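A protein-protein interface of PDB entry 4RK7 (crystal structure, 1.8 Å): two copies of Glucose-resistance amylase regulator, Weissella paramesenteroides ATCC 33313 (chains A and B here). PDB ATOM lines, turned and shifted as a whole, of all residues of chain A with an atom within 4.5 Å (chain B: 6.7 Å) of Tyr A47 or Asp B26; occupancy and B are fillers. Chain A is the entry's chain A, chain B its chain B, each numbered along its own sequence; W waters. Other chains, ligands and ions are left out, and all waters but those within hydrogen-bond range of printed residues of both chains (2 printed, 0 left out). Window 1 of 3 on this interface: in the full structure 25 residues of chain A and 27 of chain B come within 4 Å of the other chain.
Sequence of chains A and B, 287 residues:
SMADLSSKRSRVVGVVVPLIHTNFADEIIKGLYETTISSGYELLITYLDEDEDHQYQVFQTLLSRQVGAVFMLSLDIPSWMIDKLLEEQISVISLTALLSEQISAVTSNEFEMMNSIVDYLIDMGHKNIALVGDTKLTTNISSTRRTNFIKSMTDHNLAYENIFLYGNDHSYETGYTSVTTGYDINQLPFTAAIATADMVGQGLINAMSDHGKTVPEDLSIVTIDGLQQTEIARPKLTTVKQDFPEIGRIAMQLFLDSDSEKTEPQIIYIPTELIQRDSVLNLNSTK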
ATOM      1  N   VAL A  17      19.649  -5.644  24.977  1.00  0.00           N
ATOM      2  CA  VAL A  17      20.178  -4.534  25.757  1.00  0.00           C
ATOM      3  C   VAL A  17      18.994  -3.752  26.340  1.00  0.00           C
ATOM      4  O   VAL A  17      18.017  -3.505  25.641  1.00  0.00           O
ATOM      5  CB  VAL A  17      20.998  -3.593  24.843  1.00  0.00           C
ATOM      6  CG1 VAL A  17      21.592  -2.431  25.624  1.00  0.00           C
ATOM      7  CG2 VAL A  17      22.097  -4.376  24.125  1.00  0.00           C
ATOM      8  N   PRO A  18      19.069  -3.383  27.616  1.00  0.00           N
ATOM      9  CA  PRO A  18      17.976  -2.568  28.174  1.00  0.00           C
ATOM     10  C   PRO A  18      17.911  -1.187  27.517  1.00  0.00           C
ATOM     11  O   PRO A  18      18.955  -0.632  27.146  1.00  0.00           O
ATOM     12  CB  PRO A  18      18.346  -2.442  29.650  1.00  0.00           C
ATOM     13  CG  PRO A  18      19.811  -2.663  29.706  1.00  0.00           C
ATOM     14  CD  PRO A  18      20.167  -3.582  28.576  1.00  0.00           C
ATOM     15  N   LEU A  19      16.706  -0.648  27.344  1.00  0.00           N
ATOM     16  CA  LEU A  19      16.564   0.722  26.820  1.00  0.00           C
ATOM     17  C   LEU A  19      17.355   1.731  27.649  1.00  0.00           C
ATOM     18  O   LEU A  19      17.994   2.628  27.103  1.00  0.00           O
ATOM     19  CB  LEU A  19      15.099   1.168  26.772  1.00  0.00           C
ATOM     20  CG  LEU A  19      14.375   1.211  25.423  1.00  0.00           C
ATOM     21  CD1 LEU A  19      13.123   2.056  25.594  1.00  0.00           C
ATOM     22  CD2 LEU A  19      15.234   1.755  24.286  1.00  0.00           C
ATOM     23  N   HIS A  21      20.448   2.264  29.912  1.00  0.00           N
ATOM     24  CA  HIS A  21      21.726   1.622  30.218  1.00  0.00           C
ATOM     25  C   HIS A  21      22.866   2.621  30.347  1.00  0.00           C
ATOM     26  O   HIS A  21      22.898   3.633  29.644  1.00  0.00           O
ATOM     27  CB  HIS A  21      22.074   0.597  29.128  1.00  0.00           C
ATOM     28  CG  HIS A  21      22.137   1.174  27.745  1.00  0.00           C
ATOM     29  ND1 HIS A  21      21.009   1.450  27.001  1.00  0.00           N
ATOM     30  CD2 HIS A  21      23.191   1.519  26.968  1.00  0.00           C
ATOM     31  CE1 HIS A  21      21.365   1.943  25.829  1.00  0.00           C
ATOM     32  NE2 HIS A  21      22.684   1.994  25.782  1.00  0.00           N
ATOM     33  N   ASN A  23      26.921   3.329  29.653  1.00  0.00           N
ATOM     34  CA  ASN A  23      27.793   2.951  28.527  1.00  0.00           C
ATOM     35  C   ASN A  23      28.519   1.605  28.667  1.00  0.00           C
ATOM     36  O   ASN A  23      29.338   1.254  27.804  1.00  0.00           O
ATOM     37  CB  ASN A  23      28.817   4.060  28.229  1.00  0.00           C
ATOM     38  CG  ASN A  23      28.281   5.111  27.268  1.00  0.00           C
ATOM     39  OD1 ASN A  23      27.567   4.796  26.308  1.00  0.00           O
ATOM     40  ND2 ASN A  23      28.638   6.367  27.511  1.00  0.00           N
ATOM     41  N   THR A  46      19.210  -5.728  19.791  1.00  0.00           N
ATOM     42  CA  THR A  46      17.819  -5.367  19.954  1.00  0.00           C
ATOM     43  C   THR A  46      17.656  -4.788  21.360  1.00  0.00           C
ATOM     44  O   THR A  46      18.399  -5.133  22.288  1.00  0.00           O
ATOM     45  CB  THR A  46      16.884  -6.591  19.680  1.00  0.00           C
ATOM     46  OG1 THR A  46      15.523  -6.155  19.580  1.00  0.00           O
ATOM     47  CG2 THR A  46      17.018  -7.634  20.764  1.00  0.00           C
ATOM     48  N   TYR A  47      16.704  -3.873  21.509  1.00  0.00           N
ATOM     49  CA  TYR A  47      16.453  -3.235  22.795  1.00  0.00           C
ATOM     50  C   TYR A  47      15.211  -3.810  23.438  1.00  0.00           C
ATOM     51  O   TYR A  47      14.320  -4.347  22.764  1.00  0.00           O
ATOM     52  CB  TYR A  47      16.329  -1.712  22.650  1.00  0.00           C
ATOM     53  CG  TYR A  47      17.643  -1.080  22.293  1.00  0.00           C
ATOM     54  CD1 TYR A  47      18.593  -0.815  23.267  1.00  0.00           C
ATOM     55  CD2 TYR A  47      17.961  -0.785  20.971  1.00  0.00           C
ATOM     56  CE1 TYR A  47      19.814  -0.251  22.947  1.00  0.00           C
ATOM     57  CE2 TYR A  47      19.182  -0.224  20.639  1.00  0.00           C
ATOM     58  CZ  TYR A  47      20.105   0.041  21.630  1.00  0.00           C
ATOM     59  OH  TYR A  47      21.319   0.600  21.308  1.00  0.00           O
ATOM     60  N   LEU A  48      15.197  -3.739  24.760  1.00  0.00           N
ATOM     61  CA  LEU A  48      14.114  -4.283  25.558  1.00  0.00           C
ATOM     62  C   LEU A  48      13.641  -3.211  26.529  1.00  0.00           C
ATOM     63  O   LEU A  48      14.439  -2.693  27.331  1.00  0.00           O
ATOM     64  CB  LEU A  48      14.598  -5.490  26.349  1.00  0.00           C
ATOM     65  CG  LEU A  48      13.487  -6.341  26.963  1.00  0.00           C
ATOM     66  CD1 LEU A  48      13.134  -7.471  26.010  1.00  0.00           C
ATOM     67  CD2 LEU A  48      13.910  -6.866  28.326  1.00  0.00           C
ATOM     68  N   ASP A  49      12.349  -2.887  26.456  1.00  0.00           N
ATOM     69  CA  ASP A  49      11.731  -1.960  27.404  1.00  0.00           C
ATOM     70  C   ASP A  49      10.977  -2.766  28.475  1.00  0.00           C
ATOM     71  O   ASP A  49      11.241  -3.959  28.649  1.00  0.00           O
ATOM     72  CB  ASP A  49      10.853  -0.905  26.684  1.00  0.00           C
ATOM     73  CG  ASP A  49       9.631  -1.494  25.980  1.00  0.00           C
ATOM     74  OD1 ASP A  49       9.310  -2.689  26.147  1.00  0.00           O
ATOM     75  OD2 ASP A  49       8.972  -0.732  25.245  1.00  0.00           O
ATOM     76  N   VAL A  58       9.946  -8.569  20.332  1.00  0.00           N
ATOM     77  CA  VAL A  58      11.396  -8.738  20.363  1.00  0.00           C
ATOM     78  C   VAL A  58      11.795 -10.210  20.355  1.00  0.00           C
ATOM     79  O   VAL A  58      12.788 -10.588  19.740  1.00  0.00           O
ATOM     80  CB  VAL A  58      12.002  -8.058  21.612  1.00  0.00           C
ATOM     81  CG1 VAL A  58      13.455  -8.480  21.836  1.00  0.00           C
ATOM     82  CG2 VAL A  58      11.901  -6.552  21.486  1.00  0.00           C
ATOM     83  N   VAL B  15      18.999  -0.339  11.559  1.00  0.00           N
ATOM     84  CA  VAL B  15      19.767   0.873  11.767  1.00  0.00           C
ATOM     85  C   VAL B  15      21.245   0.483  11.779  1.00  0.00           C
ATOM     86  O   VAL B  15      21.658  -0.483  12.435  1.00  0.00           O
ATOM     87  CB  VAL B  15      19.318   1.679  13.010  1.00  0.00           C
ATOM     88  CG1 VAL B  15      19.389   0.846  14.273  1.00  0.00           C
ATOM     89  CG2 VAL B  15      20.137   2.958  13.151  1.00  0.00           C
ATOM     90  N   VAL B  17      24.925   1.638  12.615  1.00  0.00           N
ATOM     91  CA  VAL B  17      25.596   2.574  13.512  1.00  0.00           C
ATOM     92  C   VAL B  17      27.100   2.359  13.376  1.00  0.00           C
ATOM     93  O   VAL B  17      27.558   1.218  13.355  1.00  0.00           O
ATOM     94  CB  VAL B  17      25.152   2.338  14.979  1.00  0.00           C
ATOM     95  CG1 VAL B  17      25.877   3.264  15.947  1.00  0.00           C
ATOM     96  CG2 VAL B  17      23.649   2.532  15.113  1.00  0.00           C
ATOM     97  N   HIS B  21      31.345   6.117  17.663  1.00  0.00           N
ATOM     98  CA  HIS B  21      30.281   7.126  17.627  1.00  0.00           C
ATOM     99  C   HIS B  21      30.172   7.909  18.930  1.00  0.00           C
ATOM    100  O   HIS B  21      30.411   7.362  20.011  1.00  0.00           O
ATOM    101  CB  HIS B  21      28.928   6.458  17.323  1.00  0.00           C
ATOM    102  CG  HIS B  21      28.506   5.435  18.340  1.00  0.00           C
ATOM    103  ND1 HIS B  21      27.608   5.713  19.350  1.00  0.00           N
ATOM    104  CD2 HIS B  21      28.850   4.134  18.493  1.00  0.00           C
ATOM    105  CE1 HIS B  21      27.419   4.627  20.082  1.00  0.00           C
ATOM    106  NE2 HIS B  21      28.161   3.655  19.583  1.00  0.00           N
ATOM    107  N   THR B  22      29.802   9.189  18.819  1.00  0.00           N
ATOM    108  CA  THR B  22      29.368   9.976  19.976  1.00  0.00           C
ATOM    109  C   THR B  22      28.090   9.303  20.520  1.00  0.00           C
ATOM    110  O   THR B  22      27.497   8.437  19.859  1.00  0.00           O
ATOM    111  CB  THR B  22      29.079  11.471  19.604  1.00  0.00           C
ATOM    112  OG1 THR B  22      30.221  12.095  18.981  1.00  0.00           O
ATOM    113  CG2 THR B  22      28.698  12.294  20.827  1.00  0.00           C
ATOM    114  N   ASN B  23      27.680   9.687  21.728  1.00  0.00           N
ATOM    115  CA  ASN B  23      26.384   9.282  22.286  1.00  0.00           C
ATOM    116  C   ASN B  23      25.136   9.735  21.509  1.00  0.00           C
ATOM    117  O   ASN B  23      24.003   9.402  21.891  1.00  0.00           O
ATOM    118  CB  ASN B  23      26.276   9.733  23.748  1.00  0.00           C
ATOM    119  CG  ASN B  23      26.903   8.738  24.701  1.00  0.00           C
ATOM    120  OD1 ASN B  23      27.992   8.968  25.231  1.00  0.00           O
ATOM    121  ND2 ASN B  23      26.232   7.607  24.900  1.00  0.00           N
ATOM    122  N   PHE B  24      25.317  10.450  20.401  1.00  0.00           N
ATOM    123  CA  PHE B  24      24.160  10.925  19.648  1.00  0.00           C
ATOM    124  C   PHE B  24      23.309   9.782  19.093  1.00  0.00           C
ATOM    125  O   PHE B  24      22.088   9.923  18.977  1.00  0.00           O
ATOM    126  CB  PHE B  24      24.571  11.944  18.568  1.00  0.00           C
ATOM    127  CG  PHE B  24      25.004  11.341  17.263  1.00  0.00           C
ATOM    128  CD1 PHE B  24      24.078  11.067  16.280  1.00  0.00           C
ATOM    129  CD2 PHE B  24      26.339  11.093  17.000  1.00  0.00           C
ATOM    130  CE1 PHE B  24      24.459  10.531  15.061  1.00  0.00           C
ATOM    131  CE2 PHE B  24      26.732  10.541  15.787  1.00  0.00           C
ATOM    132  CZ  PHE B  24      25.792  10.264  14.814  1.00  0.00           C
ATOM    133  N   ALA B  25      23.940   8.656  18.773  1.00  0.00           N
ATOM    134  CA  ALA B  25      23.250   7.509  18.160  1.00  0.00           C
ATOM    135  C   ALA B  25      22.158   6.931  19.045  1.00  0.00           C
ATOM    136  O   ALA B  25      21.074   6.561  18.566  1.00  0.00           O
ATOM    137  CB  ALA B  25      24.251   6.419  17.802  1.00  0.00           C
ATOM    138  N   ASP B  26      22.443   6.812  20.343  1.00  0.00           N
ATOM    139  CA  ASP B  26      21.458   6.265  21.281  1.00  0.00           C
ATOM    140  C   ASP B  26      20.204   7.141  21.324  1.00  0.00           C
ATOM    141  O   ASP B  26      19.089   6.633  21.423  1.00  0.00           O
ATOM    142  CB  ASP B  26      22.050   6.146  22.698  1.00  0.00           C
ATOM    143  CG  ASP B  26      23.124   5.061  22.805  1.00  0.00           C
ATOM    144  OD1 ASP B  26      23.076   4.075  22.038  1.00  0.00           O
ATOM    145  OD2 ASP B  26      24.018   5.190  23.670  1.00  0.00           O
ATOM    146  N   GLU B  27      20.402   8.456  21.255  1.00  0.00           N
ATOM    147  CA  GLU B  27      19.282   9.389  21.283  1.00  0.00           C
ATOM    148  C   GLU B  27      18.455   9.308  20.001  1.00  0.00           C
ATOM    149  O   GLU B  27      17.230   9.360  20.051  1.00  0.00           O
ATOM    150  CB  GLU B  27      19.772  10.811  21.528  1.00  0.00           C
ATOM    151  CG  GLU B  27      20.320  11.040  22.932  1.00  0.00           C
ATOM    152  CD  GLU B  27      19.214  11.152  23.969  1.00  0.00           C
ATOM    153  OE1 GLU B  27      18.560  12.220  24.048  1.00  0.00           O
ATOM    154  OE2 GLU B  27      18.995  10.164  24.690  1.00  0.00           O
ATOM    155  N   ILE B  28      19.124   9.193  18.857  1.00  0.00           N
ATOM    156  CA  ILE B  28      18.416   8.942  17.603  1.00  0.00           C
ATOM    157  C   ILE B  28      17.614   7.657  17.709  1.00  0.00           C
ATOM    158  O   ILE B  28      16.418   7.621  17.372  1.00  0.00           O
ATOM    159  CB  ILE B  28      19.378   8.880  16.390  1.00  0.00           C
ATOM    160  CG1 ILE B  28      19.919  10.271  16.082  1.00  0.00           C
ATOM    161  CG2 ILE B  28      18.650   8.308  15.176  1.00  0.00           C
ATOM    162  CD1 ILE B  28      20.962  10.304  14.997  1.00  0.00           C
ATOM    163  N   ILE B  29      18.260   6.606  18.192  1.00  0.00           N
ATOM    164  CA  ILE B  29      17.631   5.295  18.329  1.00  0.00           C
ATOM    165  C   ILE B  29      16.431   5.307  19.276  1.00  0.00           C
ATOM    166  O   ILE B  29      15.480   4.576  19.056  1.00  0.00           O
ATOM    167  CB  ILE B  29      18.659   4.238  18.773  1.00  0.00           C
ATOM    168  CG1 ILE B  29      19.594   3.937  17.602  1.00  0.00           C
ATOM    169  CG2 ILE B  29      17.982   2.945  19.224  1.00  0.00           C
ATOM    170  CD1 ILE B  29      20.841   3.207  18.017  1.00  0.00           C
ATOM    171  N   LYS B  30      16.465   6.159  20.301  1.00  0.00           N
ATOM    172  CA  LYS B  30      15.322   6.307  21.211  1.00  0.00           C
ATOM    173  C   LYS B  30      14.100   6.750  20.408  1.00  0.00           C
ATOM    174  O   LYS B  30      13.000   6.209  20.556  1.00  0.00           O
ATOM    175  CB  LYS B  30      15.657   7.329  22.310  1.00  0.00           C
ATOM    176  CG  LYS B  30      14.519   7.685  23.256  1.00  0.00           C
ATOM    177  CD  LYS B  30      14.908   8.860  24.144  1.00  0.00           C
ATOM    178  CE  LYS B  30      13.694   9.532  24.763  1.00  0.00           C
ATOM    179  NZ  LYS B  30      14.021  10.925  25.175  1.00  0.00           N
ATOM    180  N   GLY B  31      14.308   7.733  19.542  1.00  0.00           N
ATOM    181  CA  GLY B  31      13.232   8.247  18.708  1.00  0.00           C
ATOM    182  C   GLY B  31      12.789   7.249  17.661  1.00  0.00           C
ATOM    183  O   GLY B  31      11.598   7.087  17.412  1.00  0.00           O
ATOM    184  N   TYR B  33      13.030   4.067  17.918  1.00  0.00           N
ATOM    185  CA  TYR B  33      12.382   3.026  18.699  1.00  0.00           C
ATOM    186  C   TYR B  33      10.923   3.337  19.064  1.00  0.00           C
ATOM    187  O   TYR B  33      10.043   2.484  18.909  1.00  0.00           O
ATOM    188  CB  TYR B  33      13.200   2.732  19.950  1.00  0.00           C
ATOM    189  CG  TYR B  33      12.696   1.545  20.705  1.00  0.00           C
ATOM    190  CD1 TYR B  33      12.852   0.256  20.199  1.00  0.00           C
ATOM    191  CD2 TYR B  33      12.047   1.705  21.929  1.00  0.00           C
ATOM    192  CE1 TYR B  33      12.376  -0.847  20.903  1.00  0.00           C
ATOM    193  CE2 TYR B  33      11.570   0.617  22.639  1.00  0.00           C
ATOM    194  CZ  TYR B  33      11.732  -0.654  22.132  1.00  0.00           C
ATOM    195  OH  TYR B  33      11.247  -1.715  22.864  1.00  0.00           O
ATOM    196  N   GLU B  42       9.645  -3.833  14.282  1.00  0.00           N
ATOM    197  CA  GLU B  42      10.725  -4.065  15.225  1.00  0.00           C
ATOM    198  C   GLU B  42      12.011  -3.458  14.665  1.00  0.00           C
ATOM    199  O   GLU B  42      12.157  -3.310  13.460  1.00  0.00           O
ATOM    200  CB  GLU B  42      10.890  -5.557  15.518  1.00  0.00           C
ATOM    201  CG  GLU B  42      10.859  -5.864  17.009  1.00  0.00           C
ATOM    202  CD  GLU B  42      12.059  -5.309  17.747  1.00  0.00           C
ATOM    203  OE1 GLU B  42      13.168  -5.865  17.579  1.00  0.00           O
ATOM    204  OE2 GLU B  42      11.889  -4.313  18.488  1.00  0.00           O
ATOM    205  N   LEU B  43      12.911  -3.082  15.560  1.00  0.00           N
ATOM    206  CA  LEU B  43      14.183  -2.438  15.218  1.00  0.00           C
ATOM    207  C   LEU B  43      15.374  -3.382  15.390  1.00  0.00           C
ATOM    208  O   LEU B  43      15.532  -3.983  16.435  1.00  0.00           O
ATOM    209  CB  LEU B  43      14.338  -1.230  16.125  1.00  0.00           C
ATOM    210  CG  LEU B  43      15.396  -0.180  15.842  1.00  0.00           C
ATOM    211  CD1 LEU B  43      15.182   0.400  14.458  1.00  0.00           C
ATOM    212  CD2 LEU B  43      15.311   0.898  16.911  1.00  0.00           C
ATOM    213  N   ILE B  45      19.526  -3.410  15.246  1.00  0.00           N
ATOM    214  CA  ILE B  45      20.652  -2.509  15.264  1.00  0.00           C
ATOM    215  C   ILE B  45      21.885  -3.310  14.902  1.00  0.00           C
ATOM    216  O   ILE B  45      22.104  -4.415  15.415  1.00  0.00           O
ATOM    217  CB  ILE B  45      20.835  -1.817  16.640  1.00  0.00           C
ATOM    218  CG1 ILE B  45      19.600  -0.985  16.998  1.00  0.00           C
ATOM    219  CG2 ILE B  45      22.104  -0.993  16.667  1.00  0.00           C
ATOM    220  CD1 ILE B  45      18.531  -1.750  17.747  1.00  0.00           C
ATOM    221  N   TYR B  47      26.235  -2.767  13.809  1.00  0.00           N
ATOM    222  CA  TYR B  47      27.366  -1.856  13.811  1.00  0.00           C
ATOM    223  C   TYR B  47      28.235  -2.076  12.556  1.00  0.00           C
ATOM    224  O   TYR B  47      28.274  -3.174  11.997  1.00  0.00           O
ATOM    225  CB  TYR B  47      28.191  -1.987  15.107  1.00  0.00           C
ATOM    226  CG  TYR B  47      27.474  -1.451  16.334  1.00  0.00           C
ATOM    227  CD1 TYR B  47      26.481  -2.192  16.972  1.00  0.00           C
ATOM    228  CD2 TYR B  47      27.775  -0.192  16.842  1.00  0.00           C
ATOM    229  CE1 TYR B  47      25.821  -1.697  18.087  1.00  0.00           C
ATOM    230  CE2 TYR B  47      27.121   0.312  17.955  1.00  0.00           C
ATOM    231  CZ  TYR B  47      26.145  -0.442  18.574  1.00  0.00           C
ATOM    232  OH  TYR B  47      25.490   0.056  19.678  1.00  0.00           O
ATOM    233  N   LEU B  73      23.324   6.124   9.925  1.00  0.00           N
ATOM    234  CA  LEU B  73      23.765   7.181  10.810  1.00  0.00           C
ATOM    235  C   LEU B  73      25.201   7.632  10.479  1.00  0.00           C
ATOM    236  O   LEU B  73      25.620   8.710  10.899  1.00  0.00           O
ATOM    237  CB  LEU B  73      23.654   6.680  12.263  1.00  0.00           C
ATOM    238  CG  LEU B  73      22.287   6.894  12.904  1.00  0.00           C
ATOM    239  CD1 LEU B  73      21.171   6.266  12.080  1.00  0.00           C
ATOM    240  CD2 LEU B  73      22.272   6.344  14.324  1.00  0.00           C
ATOM    241  N   PHE B 244      17.850  14.972  18.685  1.00  0.00           N
ATOM    242  CA  PHE B 244      18.143  13.672  18.082  1.00  0.00           C
ATOM    243  C   PHE B 244      16.927  12.713  18.065  1.00  0.00           C
ATOM    244  O   PHE B 244      16.669  12.053  17.052  1.00  0.00           O
ATOM    245  CB  PHE B 244      19.385  13.021  18.714  1.00  0.00           C
ATOM    246  CG  PHE B 244      20.676  13.760  18.434  1.00  0.00           C
ATOM    247  CD1 PHE B 244      21.183  13.846  17.121  1.00  0.00           C
ATOM    248  CD2 PHE B 244      21.393  14.365  19.470  1.00  0.00           C
ATOM    249  CE1 PHE B 244      22.379  14.524  16.870  1.00  0.00           C
ATOM    250  CE2 PHE B 244      22.590  15.035  19.227  1.00  0.00           C
ATOM    251  CZ  PHE B 244      23.094  15.116  17.923  1.00  0.00           C
HETATM  252  O   HOH W   1      20.661   2.810  22.294  1.00  0.00           O
HETATM  253  O   HOH W   2      14.652  -3.694  19.119  1.00  0.00           O
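The side-chain carboxylate (OE1) of Glu B42 lies within hydrogen-bond range of the side-chain hydroxyl (OG1) of Thr A46 (3.1 Å). The side-chain amide oxygen (OD1) of Asn A23 is in hydrogen-bond range of the side-chain amide nitrogen (ND2) of Asn B23, at 3.4 Å. OD2 of Asp A49 is in hydrogen-bond range of OH of Tyr B33 (3.4 Å).
The backbone NH (N) of Leu A19 sits at hydrogen-bond distance from the backbone carbonyl oxygen (O) of Leu A48, 3.1 Å away. The backbone carbonyl oxygen (O) of Thr A46 sits at hydrogen-bond distance from the backbone NH (N) of Val A17, 3.0 Å away. O of Leu A19 lies within hydrogen-bond range of ND1 of His A21 (3.2 Å).
Tyr B33 touches Leu A19. Thr A46 touches Leu B43. OD1 of Asp B26 touches OH of Tyr A47, at 3.96 Å. CE2 of Tyr A47 touches CG2 of Ile B29, 3.7 Å away. CE2 of Tyr A47 touches CD1 of Ile B45, 3.3 Å away. Val A58 touches Glu B42.
Of chain B, only Asp B26 (3.96 Å), Ile B29 (3.7 Å) and Ile B45 (3.3 Å) come within 4 Å of Tyr A47. Of chain A, only Tyr A47 (3.96 Å) comes within 4 Å of Asp B26. Printed residues of chain B within 4 Å of Thr A46: Glu B42 and Leu B43. Printed residues of chain A within 4 Å of Glu B42: Thr A46 and Val A58. Of the printed residues of chain B, Leu A19 touches Tyr B33 (3.6 Å). Printed residues of chain A within 4 Å of Leu B43: Thr A46 (3.8 Å). Val B17 touches none of the printed residues of chain A. The nearest residue of chain A that does not touch Asp B26 is His A21 (4.1 Å). The nearest printed residue of chain A that does not touch Leu B43 is Tyr A47 (5.1 Å).
Hydrophobic or aromatic side chains of chain B within 4 Å of the printed part of chain A: Ile B29, Tyr B33 and Ile B45.
Asn B23 touches its own counterpart, Asn A23. Of the 9 pairs that touch across the chains among the printed residues, 1 has its exchanged pair printed and touching as well.
Water W1 lies within hydrogen-bond range of OH of Tyr A47 and OD1 of Asp B26. Water W2 lies within hydrogen-bond range of the side-chain hydroxyl (OG1) of Thr A46 (2.7 Å), the backbone carbonyl oxygen (O) of Leu B43 (2.8 Å), the side-chain carboxylate (OE2) of Glu B42 (2.9 Å) and the backbone NH (N) of Tyr A47 (3.2 Å).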
